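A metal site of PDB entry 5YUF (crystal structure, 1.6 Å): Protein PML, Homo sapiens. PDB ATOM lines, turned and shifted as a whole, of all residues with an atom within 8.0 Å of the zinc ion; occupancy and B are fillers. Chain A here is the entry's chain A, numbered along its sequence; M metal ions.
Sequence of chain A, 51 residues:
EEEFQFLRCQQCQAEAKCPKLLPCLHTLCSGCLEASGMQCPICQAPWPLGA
The backbone carbonyl oxygen (O) of Ala 14 lies within hydrogen-bond range of the backbone NH (N) of Cys 9 (2.7 Å).
The side-chain sulfur of Cys 9 lies close to the backbone NH of Gln 11, 3.3 Å away.
The side-chain sulfur of Cys 12 lies close to the backbone NH of Ala 14 (3.4 Å).
Along chain A the residues within 4 Å of the zinc ion span positions 9 to 32.
The zinc ion is bound by SG of Cys 29, SG of Cys 32, SG of Cys 12 and SG of Cys 9.
The zinc ion has four donor atoms within binding distance.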
ATOM      1  N   ARG A   8     -22.306  15.809  -3.108  1.00  0.00           N
ATOM      2  CA  ARG A   8     -22.686  16.063  -1.718  1.00  0.00           C
ATOM      3  C   ARG A   8     -24.205  16.167  -1.584  1.00  0.00           C
ATOM      4  O   ARG A   8     -24.879  16.793  -2.413  1.00  0.00           O
ATOM      5  CB  ARG A   8     -22.041  17.361  -1.230  1.00  0.00           C
ATOM      6  CG  ARG A   8     -20.507  17.351  -1.206  1.00  0.00           C
ATOM      7  CD  ARG A   8     -19.933  16.917   0.139  1.00  0.00           C
ATOM      8  NE  ARG A   8     -19.278  15.614   0.133  1.00  0.00           N
ATOM      9  CZ  ARG A   8     -18.884  14.976   1.232  1.00  0.00           C
ATOM     10  NH1 ARG A   8     -19.047  15.544   2.426  1.00  0.00           N
ATOM     11  NH2 ARG A   8     -18.304  13.792   1.141  1.00  0.00           N
ATOM     12  N   CYS A   9     -24.738  15.581  -0.507  1.00  0.00           N
ATOM     13  CA  CYS A   9     -26.148  15.755  -0.178  1.00  0.00           C
ATOM     14  C   CYS A   9     -26.460  17.195   0.172  1.00  0.00           C
ATOM     15  O   CYS A   9     -25.777  17.804   1.009  1.00  0.00           O
ATOM     16  CB  CYS A   9     -26.520  14.846   1.000  1.00  0.00           C
ATOM     17  SG  CYS A   9     -28.245  15.011   1.515  1.00  0.00           S
ATOM     18  N   GLN A  10     -27.499  17.744  -0.435  1.00  0.00           N
ATOM     19  CA  GLN A  10     -27.886  19.120  -0.149  1.00  0.00           C
ATOM     20  C   GLN A  10     -28.712  19.255   1.130  1.00  0.00           C
ATOM     21  O   GLN A  10     -29.027  20.382   1.532  1.00  0.00           O
ATOM     22  CB  GLN A  10     -28.652  19.722  -1.320  1.00  0.00           C
ATOM     23  CG  GLN A  10     -27.828  19.882  -2.582  1.00  0.00           C
ATOM     24  CD  GLN A  10     -28.621  20.434  -3.735  1.00  0.00           C
ATOM     25  OE1 GLN A  10     -29.510  19.774  -4.266  1.00  0.00           O
ATOM     26  NE2 GLN A  10     -28.299  21.652  -4.132  1.00  0.00           N
ATOM     27  N   GLN A  11     -29.055  18.148   1.793  1.00  0.00           N
ATOM     28  CA  GLN A  11     -29.758  18.170   3.069  1.00  0.00           C
ATOM     29  C   GLN A  11     -28.818  18.104   4.259  1.00  0.00           C
ATOM     30  O   GLN A  11     -28.953  18.889   5.198  1.00  0.00           O
ATOM     31  CB  GLN A  11     -30.765  17.017   3.112  1.00  0.00           C
ATOM     32  CG  GLN A  11     -31.473  16.779   4.451  1.00  0.00           C
ATOM     33  CD  GLN A  11     -32.422  17.890   4.834  1.00  0.00           C
ATOM     34  OE1 GLN A  11     -32.714  18.781   4.039  1.00  0.00           O
ATOM     35  NE2 GLN A  11     -32.942  17.814   6.051  1.00  0.00           N
ATOM     36  N   CYS A  12     -27.863  17.176   4.246  1.00  0.00           N
ATOM     37  CA  CYS A  12     -26.958  16.953   5.373  1.00  0.00           C
ATOM     38  C   CYS A  12     -25.494  17.206   5.029  1.00  0.00           C
ATOM     39  O   CYS A  12     -24.640  17.103   5.918  1.00  0.00           O
ATOM     40  CB  CYS A  12     -27.127  15.519   5.893  1.00  0.00           C
ATOM     41  SG  CYS A  12     -26.407  14.267   4.833  1.00  0.00           S
ATOM     42  N   GLN A  13     -25.192  17.545   3.767  1.00  0.00           N
ATOM     43  CA  GLN A  13     -23.847  17.764   3.233  1.00  0.00           C
ATOM     44  C   GLN A  13     -22.909  16.557   3.444  1.00  0.00           C
ATOM     45  O   GLN A  13     -21.693  16.704   3.303  1.00  0.00           O
ATOM     46  CB  GLN A  13     -23.181  19.040   3.770  1.00  0.00           C
ATOM     47  CG  GLN A  13     -23.852  19.811   4.902  1.00  0.00           C
ATOM     48  CD  GLN A  13     -25.242  20.323   4.552  1.00  0.00           C
ATOM     49  OE1 GLN A  13     -25.547  20.610   3.398  1.00  0.00           O
ATOM     50  NE2 GLN A  13     -26.099  20.423   5.568  1.00  0.00           N
ATOM     51  N   ALA A  14     -23.432  15.370   3.729  1.00  0.00           N
ATOM     52  CA  ALA A  14     -22.602  14.175   3.614  1.00  0.00           C
ATOM     53  C   ALA A  14     -22.409  13.827   2.143  1.00  0.00           C
ATOM     54  O   ALA A  14     -22.974  14.443   1.242  1.00  0.00           O
ATOM     55  CB  ALA A  14     -23.245  13.015   4.362  1.00  0.00           C
ATOM     56  N   GLU A  15     -21.572  12.812   1.891  1.00  0.00           N
ATOM     57  CA  GLU A  15     -21.398  12.320   0.526  1.00  0.00           C
ATOM     58  C   GLU A  15     -22.699  11.712   0.019  1.00  0.00           C
ATOM     59  O   GLU A  15     -23.409  11.025   0.755  1.00  0.00           O
ATOM     60  CB  GLU A  15     -20.279  11.275   0.464  1.00  0.00           C
ATOM     61  CG  GLU A  15     -19.747  11.034  -0.944  1.00  0.00           C
ATOM     62  CD  GLU A  15     -18.581  10.062  -0.973  1.00  0.00           C
ATOM     63  OE1 GLU A  15     -17.554  10.381  -1.623  1.00  0.00           O
ATOM     64  OE2 GLU A  15     -18.633   9.038  -0.256  1.00  0.00           O
ATOM     65  N   ALA A  16     -23.009  11.977  -1.248  1.00  0.00           N
ATOM     66  CA  ALA A  16     -24.130  11.343  -1.948  1.00  0.00           C
ATOM     67  C   ALA A  16     -23.528  10.670  -3.173  1.00  0.00           C
ATOM     68  O   ALA A  16     -23.389  11.281  -4.237  1.00  0.00           O
ATOM     69  CB  ALA A  16     -25.220  12.350  -2.302  1.00  0.00           C
ATOM     70  N   THR A  27     -30.279  17.153  -4.805  1.00  0.00           N
ATOM     71  CA  THR A  27     -29.393  16.011  -4.640  1.00  0.00           C
ATOM     72  C   THR A  27     -29.464  15.552  -3.188  1.00  0.00           C
ATOM     73  O   THR A  27     -29.192  16.343  -2.275  1.00  0.00           O
ATOM     74  CB  THR A  27     -27.957  16.380  -5.001  1.00  0.00           C
ATOM     75  OG1 THR A  27     -27.890  16.803  -6.359  1.00  0.00           O
ATOM     76  CG2 THR A  27     -27.031  15.186  -4.821  1.00  0.00           C
ATOM     77  N   LEU A  28     -29.834  14.290  -2.957  1.00  0.00           N
ATOM     78  CA  LEU A  28     -29.941  13.732  -1.616  1.00  0.00           C
ATOM     79  C   LEU A  28     -29.114  12.459  -1.494  1.00  0.00           C
ATOM     80  O   LEU A  28     -29.040  11.677  -2.438  1.00  0.00           O
ATOM     81  CB  LEU A  28     -31.385  13.412  -1.260  1.00  0.00           C
ATOM     82  CG  LEU A  28     -32.373  14.573  -1.276  1.00  0.00           C
ATOM     83  CD1 LEU A  28     -33.781  14.084  -0.959  1.00  0.00           C
ATOM     84  CD2 LEU A  28     -31.944  15.653  -0.311  1.00  0.00           C
ATOM     85  N   CYS A  29     -28.485  12.256  -0.335  1.00  0.00           N
ATOM     86  CA  CYS A  29     -27.904  10.968  -0.017  1.00  0.00           C
ATOM     87  C   CYS A  29     -29.012   9.941   0.226  1.00  0.00           C
ATOM     88  O   CYS A  29     -30.189  10.278   0.366  1.00  0.00           O
ATOM     89  CB  CYS A  29     -26.990  11.058   1.207  1.00  0.00           C
ATOM     90  SG  CYS A  29     -27.832  11.335   2.792  1.00  0.00           S
ATOM     91  N   SER A  30     -28.634   8.662   0.237  1.00  0.00           N
ATOM     92  CA  SER A  30     -29.629   7.603   0.363  1.00  0.00           C
ATOM     93  C   SER A  30     -30.348   7.670   1.701  1.00  0.00           C
ATOM     94  O   SER A  30     -31.554   7.437   1.774  1.00  0.00           O
ATOM     95  CB  SER A  30     -28.972   6.243   0.164  1.00  0.00           C
ATOM     96  OG  SER A  30     -27.940   6.033   1.111  1.00  0.00           O
ATOM     97  N   GLY A  31     -29.612   7.970   2.774  1.00  0.00           N
ATOM     98  CA  GLY A  31     -30.245   8.111   4.087  1.00  0.00           C
ATOM     99  C   GLY A  31     -31.313   9.180   4.111  1.00  0.00           C
ATOM    100  O   GLY A  31     -32.424   8.957   4.611  1.00  0.00           O
ATOM    101  N   CYS A  32     -30.979  10.384   3.626  1.00  0.00           N
ATOM    102  CA  CYS A  32     -31.944  11.469   3.611  1.00  0.00           C
ATOM    103  C   CYS A  32     -33.141  11.143   2.709  1.00  0.00           C
ATOM    104  O   CYS A  32     -34.276  11.502   3.024  1.00  0.00           O
ATOM    105  CB  CYS A  32     -31.256  12.768   3.174  1.00  0.00           C
ATOM    106  SG  CYS A  32     -30.162  13.502   4.461  1.00  0.00           S
ATOM    107  N   LEU A  33     -32.911  10.437   1.595  1.00  0.00           N
ATOM    108  CA  LEU A  33     -34.040  10.054   0.762  1.00  0.00           C
ATOM    109  C   LEU A  33     -34.928   9.049   1.493  1.00  0.00           C
ATOM    110  O   LEU A  33     -36.155   9.161   1.474  1.00  0.00           O
ATOM    111  CB  LEU A  33     -33.537   9.494  -0.576  1.00  0.00           C
ATOM    112  CG  LEU A  33     -34.598   9.176  -1.615  1.00  0.00           C
ATOM    113  CD1 LEU A  33     -35.443  10.400  -1.932  1.00  0.00           C
ATOM    114  CD2 LEU A  33     -33.959   8.656  -2.884  1.00  0.00           C
ATOM    115  N   PRO A  41     -37.152  16.928   1.577  1.00  0.00           N
ATOM    116  CA  PRO A  41     -36.900  17.637   2.849  1.00  0.00           C
ATOM    117  C   PRO A  41     -36.430  19.059   2.665  1.00  0.00           C
ATOM    118  O   PRO A  41     -36.474  19.823   3.630  1.00  0.00           O
ATOM    119  CB  PRO A  41     -35.810  16.776   3.509  1.00  0.00           C
ATOM    120  CG  PRO A  41     -35.117  16.113   2.357  1.00  0.00           C
ATOM    121  CD  PRO A  41     -36.177  15.871   1.321  1.00  0.00           C
HETATM  122 ZN    ZN M   1     -28.097  13.469   3.407  1.00  0.00          ZN
